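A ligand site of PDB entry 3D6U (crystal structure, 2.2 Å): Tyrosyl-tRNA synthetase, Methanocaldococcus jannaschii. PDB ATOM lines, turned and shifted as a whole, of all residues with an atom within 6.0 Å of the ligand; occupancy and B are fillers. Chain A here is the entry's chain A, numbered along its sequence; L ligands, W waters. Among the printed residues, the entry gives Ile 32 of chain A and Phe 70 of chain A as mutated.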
ATOM      1  N   ILE A  32      11.249  14.401 -13.052  1.00  0.00           N
ATOM      2  CA  ILE A  32      10.103  14.166 -12.212  1.00  0.00           C
ATOM      3  C   ILE A  32       8.837  14.284 -13.029  1.00  0.00           C
ATOM      4  O   ILE A  32       8.780  15.033 -14.000  1.00  0.00           O
ATOM      5  CB  ILE A  32      10.060  15.234 -11.033  1.00  0.00           C
ATOM      6  CG1 ILE A  32       9.049  14.792  -9.959  1.00  0.00           C
ATOM      7  CG2 ILE A  32       9.776  16.667 -11.601  1.00  0.00           C
ATOM      8  CD1 ILE A  32       9.366  15.279  -8.557  1.00  0.00           C
ATOM      9  N   ILE A  33       7.800  13.604 -12.562  1.00  0.00           N
ATOM     10  CA  ILE A  33       6.456  13.850 -12.996  1.00  0.00           C
ATOM     11  C   ILE A  33       5.534  13.709 -11.789  1.00  0.00           C
ATOM     12  O   ILE A  33       5.776  12.844 -10.925  1.00  0.00           O
ATOM     13  CB  ILE A  33       6.000  12.962 -14.172  1.00  0.00           C
ATOM     14  CG1 ILE A  33       4.543  13.321 -14.557  1.00  0.00           C
ATOM     15  CG2 ILE A  33       6.163  11.470 -13.895  1.00  0.00           C
ATOM     16  CD1 ILE A  33       4.153  12.762 -16.026  1.00  0.00           C
ATOM     17  N   GLY A  34       4.488  14.545 -11.711  1.00  0.00           N
ATOM     18  CA  GLY A  34       3.474  14.300 -10.678  1.00  0.00           C
ATOM     19  C   GLY A  34       2.147  13.864 -11.197  1.00  0.00           C
ATOM     20  O   GLY A  34       1.693  14.324 -12.260  1.00  0.00           O
ATOM     21  N   PHE A  35       1.479  13.021 -10.397  1.00  0.00           N
ATOM     22  CA  PHE A  35       0.131  12.550 -10.724  1.00  0.00           C
ATOM     23  C   PHE A  35      -0.772  12.613  -9.540  1.00  0.00           C
ATOM     24  O   PHE A  35      -0.477  12.000  -8.517  1.00  0.00           O
ATOM     25  CB  PHE A  35       0.107  11.054 -11.122  1.00  0.00           C
ATOM     26  CG  PHE A  35       0.741  10.748 -12.403  1.00  0.00           C
ATOM     27  CD1 PHE A  35       2.014  10.185 -12.442  1.00  0.00           C
ATOM     28  CD2 PHE A  35       0.081  11.007 -13.591  1.00  0.00           C
ATOM     29  CE1 PHE A  35       2.601   9.866 -13.669  1.00  0.00           C
ATOM     30  CE2 PHE A  35       0.679  10.722 -14.822  1.00  0.00           C
ATOM     31  CZ  PHE A  35       1.918  10.150 -14.871  1.00  0.00           C
ATOM     32  N   GLU A  36      -1.913  13.304  -9.667  1.00  0.00           N
ATOM     33  CA  GLU A  36      -3.012  13.088  -8.711  1.00  0.00           C
ATOM     34  C   GLU A  36      -3.463  11.598  -8.833  1.00  0.00           C
ATOM     35  O   GLU A  36      -3.718  11.108  -9.949  1.00  0.00           O
ATOM     36  CB  GLU A  36      -4.197  14.015  -9.022  1.00  0.00           C
ATOM     37  CG  GLU A  36      -3.939  15.525  -8.851  1.00  0.00           C
ATOM     38  CD  GLU A  36      -5.191  16.295  -9.202  1.00  0.00           C
ATOM     39  OE1 GLU A  36      -6.245  15.768  -8.843  1.00  0.00           O
ATOM     40  OE2 GLU A  36      -5.180  17.384  -9.812  1.00  0.00           O
ATOM     41  N   LEU A  65       5.926  11.689  -8.271  1.00  0.00           N
ATOM     42  CA  LEU A  65       5.180  12.246  -7.166  1.00  0.00           C
ATOM     43  C   LEU A  65       3.743  11.794  -7.251  1.00  0.00           C
ATOM     44  O   LEU A  65       3.044  12.028  -8.233  1.00  0.00           O
ATOM     45  CB  LEU A  65       5.253  13.764  -7.174  1.00  0.00           C
ATOM     46  CG  LEU A  65       4.496  14.390  -5.994  1.00  0.00           C
ATOM     47  CD1 LEU A  65       5.319  14.158  -4.703  1.00  0.00           C
ATOM     48  CD2 LEU A  65       4.318  15.797  -6.369  1.00  0.00           C
ATOM     49  N   ALA A  67       0.769  12.646  -6.193  1.00  0.00           N
ATOM     50  CA  ALA A  67       0.494  14.049  -5.736  1.00  0.00           C
ATOM     51  C   ALA A  67      -0.761  14.084  -4.862  1.00  0.00           C
ATOM     52  O   ALA A  67      -1.782  14.645  -5.233  1.00  0.00           O
ATOM     53  CB  ALA A  67       0.336  14.948  -6.917  1.00  0.00           C
ATOM     54  N   PHE A  70      -2.201  17.481  -3.595  1.00  0.00           N
ATOM     55  CA  PHE A  70      -2.717  18.085  -4.811  1.00  0.00           C
ATOM     56  C   PHE A  70      -4.132  17.564  -5.093  1.00  0.00           C
ATOM     57  O   PHE A  70      -5.084  18.325  -5.260  1.00  0.00           O
ATOM     58  CB  PHE A  70      -1.758  17.893  -6.025  1.00  0.00           C
ATOM     59  CG  PHE A  70      -0.452  18.679  -5.924  1.00  0.00           C
ATOM     60  CD1 PHE A  70      -0.356  19.986  -6.419  1.00  0.00           C
ATOM     61  CD2 PHE A  70       0.687  18.130  -5.329  1.00  0.00           C
ATOM     62  CE1 PHE A  70       0.844  20.732  -6.340  1.00  0.00           C
ATOM     63  CE2 PHE A  70       1.889  18.881  -5.214  1.00  0.00           C
ATOM     64  CZ  PHE A  70       1.953  20.184  -5.771  1.00  0.00           C
ATOM     65  N   TYR A 114       8.485  23.871   3.321  1.00  0.00           N
ATOM     66  CA  TYR A 114       7.568  23.717   2.202  1.00  0.00           C
ATOM     67  C   TYR A 114       6.446  24.758   2.355  1.00  0.00           C
ATOM     68  O   TYR A 114       6.169  25.539   1.425  1.00  0.00           O
ATOM     69  CB  TYR A 114       6.992  22.297   2.128  1.00  0.00           C
ATOM     70  CG  TYR A 114       6.184  22.123   0.849  1.00  0.00           C
ATOM     71  CD1 TYR A 114       6.777  21.649  -0.283  1.00  0.00           C
ATOM     72  CD2 TYR A 114       4.811  22.524   0.786  1.00  0.00           C
ATOM     73  CE1 TYR A 114       6.048  21.532  -1.492  1.00  0.00           C
ATOM     74  CE2 TYR A 114       4.086  22.420  -0.404  1.00  0.00           C
ATOM     75  CZ  TYR A 114       4.724  21.955  -1.514  1.00  0.00           C
ATOM     76  OH  TYR A 114       3.987  21.813  -2.624  1.00  0.00           O
ATOM     77  N   ILE A 137      -7.152  22.081 -15.168  1.00  0.00           N
ATOM     78  CA  ILE A 137      -6.794  21.118 -14.111  1.00  0.00           C
ATOM     79  C   ILE A 137      -7.922  21.018 -13.070  1.00  0.00           C
ATOM     80  O   ILE A 137      -8.318  19.930 -12.649  1.00  0.00           O
ATOM     81  CB  ILE A 137      -5.397  21.548 -13.462  1.00  0.00           C
ATOM     82  CG1 ILE A 137      -4.301  21.466 -14.538  1.00  0.00           C
ATOM     83  CG2 ILE A 137      -5.043  20.713 -12.245  1.00  0.00           C
ATOM     84  CD1 ILE A 137      -3.298  22.462 -14.447  1.00  0.00           C
ATOM     85  N   TYR A 151      -3.292  25.170  -5.035  1.00  0.00           N
ATOM     86  CA  TYR A 151      -2.768  24.073  -5.869  1.00  0.00           C
ATOM     87  C   TYR A 151      -1.598  24.530  -6.790  1.00  0.00           C
ATOM     88  O   TYR A 151      -0.557  23.924  -6.749  1.00  0.00           O
ATOM     89  CB  TYR A 151      -3.907  23.459  -6.646  1.00  0.00           C
ATOM     90  CG  TYR A 151      -3.656  22.252  -7.448  1.00  0.00           C
ATOM     91  CD1 TYR A 151      -4.293  21.053  -7.147  1.00  0.00           C
ATOM     92  CD2 TYR A 151      -2.854  22.304  -8.569  1.00  0.00           C
ATOM     93  CE1 TYR A 151      -4.120  19.934  -7.964  1.00  0.00           C
ATOM     94  CE2 TYR A 151      -2.655  21.168  -9.368  1.00  0.00           C
ATOM     95  CZ  TYR A 151      -3.306  20.028  -9.085  1.00  0.00           C
ATOM     96  OH  TYR A 151      -3.129  18.960  -9.866  1.00  0.00           O
ATOM     97  N   MET A 154       1.594  25.400  -5.041  1.00  0.00           N
ATOM     98  CA  MET A 154       2.293  24.245  -4.483  1.00  0.00           C
ATOM     99  C   MET A 154       3.040  23.617  -5.632  1.00  0.00           C
ATOM    100  O   MET A 154       4.186  23.298  -5.463  1.00  0.00           O
ATOM    101  CB  MET A 154       1.363  23.221  -3.884  1.00  0.00           C
ATOM    102  CG  MET A 154       0.921  23.578  -2.496  1.00  0.00           C
ATOM    103  SD  MET A 154      -0.368  22.394  -2.192  1.00  0.00           S
ATOM    104  CE  MET A 154      -0.406  22.428  -0.453  1.00  0.00           C
ATOM    105  N   GLN A 155       2.409  23.551  -6.813  1.00  0.00           N
ATOM    106  CA  GLN A 155       3.063  22.927  -7.985  1.00  0.00           C
ATOM    107  C   GLN A 155       4.358  23.633  -8.470  1.00  0.00           C
ATOM    108  O   GLN A 155       5.202  23.026  -9.104  1.00  0.00           O
ATOM    109  CB  GLN A 155       2.081  22.661  -9.144  1.00  0.00           C
ATOM    110  CG  GLN A 155       2.760  21.946 -10.332  1.00  0.00           C
ATOM    111  CD  GLN A 155       1.781  21.303 -11.212  1.00  0.00           C
ATOM    112  OE1 GLN A 155       0.711  20.936 -10.769  1.00  0.00           O
ATOM    113  NE2 GLN A 155       2.104  21.183 -12.494  1.00  0.00           N
ATOM    114  N   VAL A 156       4.543  24.900  -8.078  1.00  0.00           N
ATOM    115  CA  VAL A 156       5.646  25.733  -8.519  1.00  0.00           C
ATOM    116  C   VAL A 156       6.701  25.893  -7.378  1.00  0.00           C
ATOM    117  O   VAL A 156       7.691  26.631  -7.501  1.00  0.00           O
ATOM    118  CB  VAL A 156       4.942  27.016  -9.073  1.00  0.00           C
ATOM    119  CG1 VAL A 156       5.605  28.309  -8.802  1.00  0.00           C
ATOM    120  CG2 VAL A 156       4.487  26.835 -10.562  1.00  0.00           C
ATOM    121  N   ASN A 157       6.470  25.198  -6.256  1.00  0.00           N
ATOM    122  CA  ASN A 157       7.262  25.277  -5.101  1.00  0.00           C
ATOM    123  C   ASN A 157       8.653  24.655  -5.408  1.00  0.00           C
ATOM    124  O   ASN A 157       8.726  23.521  -5.889  1.00  0.00           O
ATOM    125  CB  ASN A 157       6.530  24.543  -3.936  1.00  0.00           C
ATOM    126  CG  ASN A 157       7.192  24.756  -2.558  1.00  0.00           C
ATOM    127  OD1 ASN A 157       8.391  24.826  -2.476  1.00  0.00           O
ATOM    128  ND2 ASN A 157       6.419  24.831  -1.496  1.00  0.00           N
ATOM    129  N   HIS A 160       9.866  20.933  -4.719  1.00  0.00           N
ATOM    130  CA  HIS A 160       9.586  19.836  -5.568  1.00  0.00           C
ATOM    131  C   HIS A 160      10.674  19.552  -6.561  1.00  0.00           C
ATOM    132  O   HIS A 160      10.696  18.456  -7.088  1.00  0.00           O
ATOM    133  CB  HIS A 160       8.274  20.043  -6.372  1.00  0.00           C
ATOM    134  CG  HIS A 160       7.044  19.986  -5.537  1.00  0.00           C
ATOM    135  ND1 HIS A 160       6.634  18.851  -4.883  1.00  0.00           N
ATOM    136  CD2 HIS A 160       6.150  20.951  -5.209  1.00  0.00           C
ATOM    137  CE1 HIS A 160       5.513  19.088  -4.229  1.00  0.00           C
ATOM    138  NE2 HIS A 160       5.194  20.370  -4.416  1.00  0.00           N
ATOM    139  N   TYR A 161      11.456  20.573  -6.892  1.00  0.00           N
ATOM    140  CA  TYR A 161      12.400  20.541  -8.022  1.00  0.00           C
ATOM    141  C   TYR A 161      13.858  20.578  -7.594  1.00  0.00           C
ATOM    142  O   TYR A 161      14.734  20.744  -8.461  1.00  0.00           O
ATOM    143  CB  TYR A 161      12.111  21.670  -9.035  1.00  0.00           C
ATOM    144  CG  TYR A 161      10.700  21.581  -9.524  1.00  0.00           C
ATOM    145  CD1 TYR A 161      10.324  20.615 -10.504  1.00  0.00           C
ATOM    146  CD2 TYR A 161       9.696  22.389  -8.940  1.00  0.00           C
ATOM    147  CE1 TYR A 161       8.967  20.501 -10.886  1.00  0.00           C
ATOM    148  CE2 TYR A 161       8.350  22.276  -9.354  1.00  0.00           C
ATOM    149  CZ  TYR A 161       8.003  21.339 -10.293  1.00  0.00           C
ATOM    150  OH  TYR A 161       6.678  21.225 -10.625  1.00  0.00           O
ATOM    151  N   ALA A 167      11.112  18.281 -15.655  1.00  0.00           N
ATOM    152  CA  ALA A 167       9.795  17.889 -15.226  1.00  0.00           C
ATOM    153  C   ALA A 167       9.019  17.576 -16.477  1.00  0.00           C
ATOM    154  O   ALA A 167       9.103  18.273 -17.496  1.00  0.00           O
ATOM    155  CB  ALA A 167       9.111  19.042 -14.410  1.00  0.00           C
ATOM    156  N   VAL A 168       8.212  16.541 -16.379  1.00  0.00           N
ATOM    157  CA  VAL A 168       7.400  16.109 -17.514  1.00  0.00           C
ATOM    158  C   VAL A 168       5.947  16.279 -17.129  1.00  0.00           C
ATOM    159  O   VAL A 168       5.609  16.063 -15.974  1.00  0.00           O
ATOM    160  CB  VAL A 168       7.743  14.654 -17.796  1.00  0.00           C
ATOM    161  CG1 VAL A 168       6.928  14.143 -18.935  1.00  0.00           C
ATOM    162  CG2 VAL A 168       9.345  14.533 -18.092  1.00  0.00           C
ATOM    163  N   GLU A 172      -1.828  20.271 -20.649  1.00  0.00           N
ATOM    164  CA  GLU A 172      -2.754  20.959 -19.720  1.00  0.00           C
ATOM    165  C   GLU A 172      -1.989  21.588 -18.532  1.00  0.00           C
ATOM    166  O   GLU A 172      -2.484  22.531 -17.845  1.00  0.00           O
ATOM    167  CB  GLU A 172      -3.884  20.037 -19.247  1.00  0.00           C
ATOM    168  CG  GLU A 172      -3.510  19.055 -18.119  1.00  0.00           C
ATOM    169  CD  GLU A 172      -2.673  17.826 -18.580  1.00  0.00           C
ATOM    170  OE1 GLU A 172      -2.478  17.660 -19.813  1.00  0.00           O
ATOM    171  OE2 GLU A 172      -2.217  17.015 -17.693  1.00  0.00           O
ATOM    172  N   GLN A 173      -0.738  21.164 -18.308  1.00  0.00           N
ATOM    173  CA  GLN A 173       0.038  21.756 -17.215  1.00  0.00           C
ATOM    174  C   GLN A 173       0.838  22.977 -17.605  1.00  0.00           C
ATOM    175  O   GLN A 173       1.497  23.523 -16.761  1.00  0.00           O
ATOM    176  CB  GLN A 173       1.030  20.747 -16.568  1.00  0.00           C
ATOM    177  CG  GLN A 173       0.455  19.403 -16.315  1.00  0.00           C
ATOM    178  CD  GLN A 173      -0.514  19.383 -15.136  1.00  0.00           C
ATOM    179  OE1 GLN A 173      -0.254  20.030 -14.080  1.00  0.00           O
ATOM    180  NE2 GLN A 173      -1.639  18.609 -15.295  1.00  0.00           N
ATOM    181  N   ILE A 176       0.674  26.398 -15.464  1.00  0.00           N
ATOM    182  CA  ILE A 176       1.391  26.230 -14.169  1.00  0.00           C
ATOM    183  C   ILE A 176       2.909  26.214 -14.394  1.00  0.00           C
ATOM    184  O   ILE A 176       3.677  26.844 -13.663  1.00  0.00           O
ATOM    185  CB  ILE A 176       0.994  24.966 -13.452  1.00  0.00           C
ATOM    186  CG1 ILE A 176      -0.501  25.065 -12.994  1.00  0.00           C
ATOM    187  CG2 ILE A 176       1.943  24.733 -12.299  1.00  0.00           C
ATOM    188  CD1 ILE A 176      -1.146  23.804 -12.434  1.00  0.00           C
ATOM    189  N   HIS A 177       3.373  25.512 -15.418  1.00  0.00           N
ATOM    190  CA  HIS A 177       4.798  25.496 -15.702  1.00  0.00           C
ATOM    191  C   HIS A 177       5.367  26.780 -16.173  1.00  0.00           C
ATOM    192  O   HIS A 177       6.501  27.057 -15.868  1.00  0.00           O
ATOM    193  CB  HIS A 177       5.106  24.374 -16.656  1.00  0.00           C
ATOM    194  CG  HIS A 177       4.848  23.050 -16.037  1.00  0.00           C
ATOM    195  ND1 HIS A 177       4.725  21.884 -16.773  1.00  0.00           N
ATOM    196  CD2 HIS A 177       4.684  22.722 -14.743  1.00  0.00           C
ATOM    197  CE1 HIS A 177       4.499  20.882 -15.941  1.00  0.00           C
ATOM    198  NE2 HIS A 177       4.471  21.367 -14.700  1.00  0.00           N
HETATM  199  F1  LIG L   1       7.259  17.886  -8.875  1.00  0.00           F
HETATM  200  C1  LIG L   1       6.122  17.664  -9.511  1.00  0.00           C
HETATM  201  F2  LIG L   1       6.365  17.801 -10.773  1.00  0.00           F
HETATM  202  F3  LIG L   1       5.743  16.420  -9.362  1.00  0.00           F
HETATM  203  C2  LIG L   1       4.997  18.661  -9.201  1.00  0.00           C
HETATM  204  N1  LIG L   1       5.351  19.971  -8.698  1.00  0.00           N
HETATM  205  N2  LIG L   1       4.894  19.173  -7.858  1.00  0.00           N
HETATM  206  C3  LIG L   1       3.616  18.218  -9.541  1.00  0.00           C
HETATM  207  C4  LIG L   1       2.649  17.991  -8.571  1.00  0.00           C
HETATM  208  C5  LIG L   1       1.384  17.552  -8.982  1.00  0.00           C
HETATM  209  C6  LIG L   1       1.111  17.388 -10.337  1.00  0.00           C
HETATM  210  C7  LIG L   1       2.094  17.633 -11.307  1.00  0.00           C
HETATM  211  C8  LIG L   1       3.336  18.066 -10.891  1.00  0.00           C
HETATM  212  C9  LIG L   1      -0.264  16.929 -10.784  1.00  0.00           C
HETATM  213  C10 LIG L   1      -0.731  17.700 -11.992  1.00  0.00           C
HETATM  214  N3  LIG L   1      -1.036  19.106 -11.728  1.00  0.00           N
HETATM  215  C11 LIG L   1      -2.003  17.024 -12.438  1.00  0.00           C
HETATM  216  O1  LIG L   1      -2.846  17.727 -13.074  1.00  0.00           O
HETATM  217  O2  LIG L   1      -2.150  15.824 -12.101  1.00  0.00           O
HETATM  218  O   HOH W   1       5.559  19.600 -12.904  1.00  0.00           O
HETATM  219  O   HOH W   2       4.474  16.978 -13.741  1.00  0.00           O
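A nitrogen (N3) of the ligand sits close to the side-chain amide oxygen (OE1) of Gln 155 (2.7 Å). A nitrogen (N3) of the ligand lies close to the side-chain hydroxyl (OH) of Tyr 151 (2.8 Å). A nitrogen (N1) of the ligand lies close to the side-chain hydroxyl (OH) of Tyr 161, 2.7 Å away. N1 of the ligand lies close to O of Gln 155 (3.1 Å). A nitrogen (N3) of the ligand lies close to the side-chain amide oxygen (OE1) of Gln 173 (2.6 Å). A ring nitrogen (ND1) of His 160 sits close to a nitrogen (N2) of the ligand.
The backbone carbonyl oxygen (O) of Ile 33 is in hydrogen-bond range of the backbone NH (N) of Leu 65, 2.9 Å away. OH of Tyr 161 lies within hydrogen-bond range of O of Gln 155 (2.8 Å). NE2 of Gln 155 sits at hydrogen-bond distance from NE2 of His 177 (3.2 Å). The side-chain amide nitrogen of Gln 173 lies within hydrogen-bond range of the side-chain carboxylate of Glu 172 (2.9 Å). The side-chain amide oxygen of Gln 173 is in hydrogen-bond range of the side-chain amide nitrogen of Gln 155 (3.1 Å). OH of Tyr 151 is in hydrogen-bond range of OE2 of Glu 36, at 2.6 Å. A ring nitrogen (NE2) of His 160 lies within hydrogen-bond range of the side-chain hydroxyl (OH) of Tyr 114 (2.6 Å). The backbone carbonyl oxygen (O) of Ile 32 sits at hydrogen-bond distance from the backbone NH (N) of Val 168.
The backbone NH (N) of Gly 34 sits close to a fluorine (F3) of the ligand. Ile 32 touches the ligand. Ile 33 touches the ligand (C to F3, 3.6 Å). N of Glu 36 touches O2 of the ligand (3.5 Å). Leu 65 touches the ligand. Ala 67 touches the ligand. Phe 70 touches the ligand (CE2 to C4, 3.6 Å). Ile 137 touches the ligand (CG2 to O1, 3.8 Å). Hydrophobic or aromatic side chains that line the ligand: Ile 32, Leu 65, Ala 67, Phe 70, Ile 137, Tyr 151, His 160 and Tyr 161. Of the 23 residues printed, 13 come within 4 Å of the ligand.
Water W1 lies within hydrogen-bond range of NE2 of His 177 (2.7 Å) and OH of Tyr 161 (3.0 Å). Water W2 bridges the backbone carbonyl oxygen of Val 168 (2.7 Å) and the backbone NH of Gly 34 (3.2 Å).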
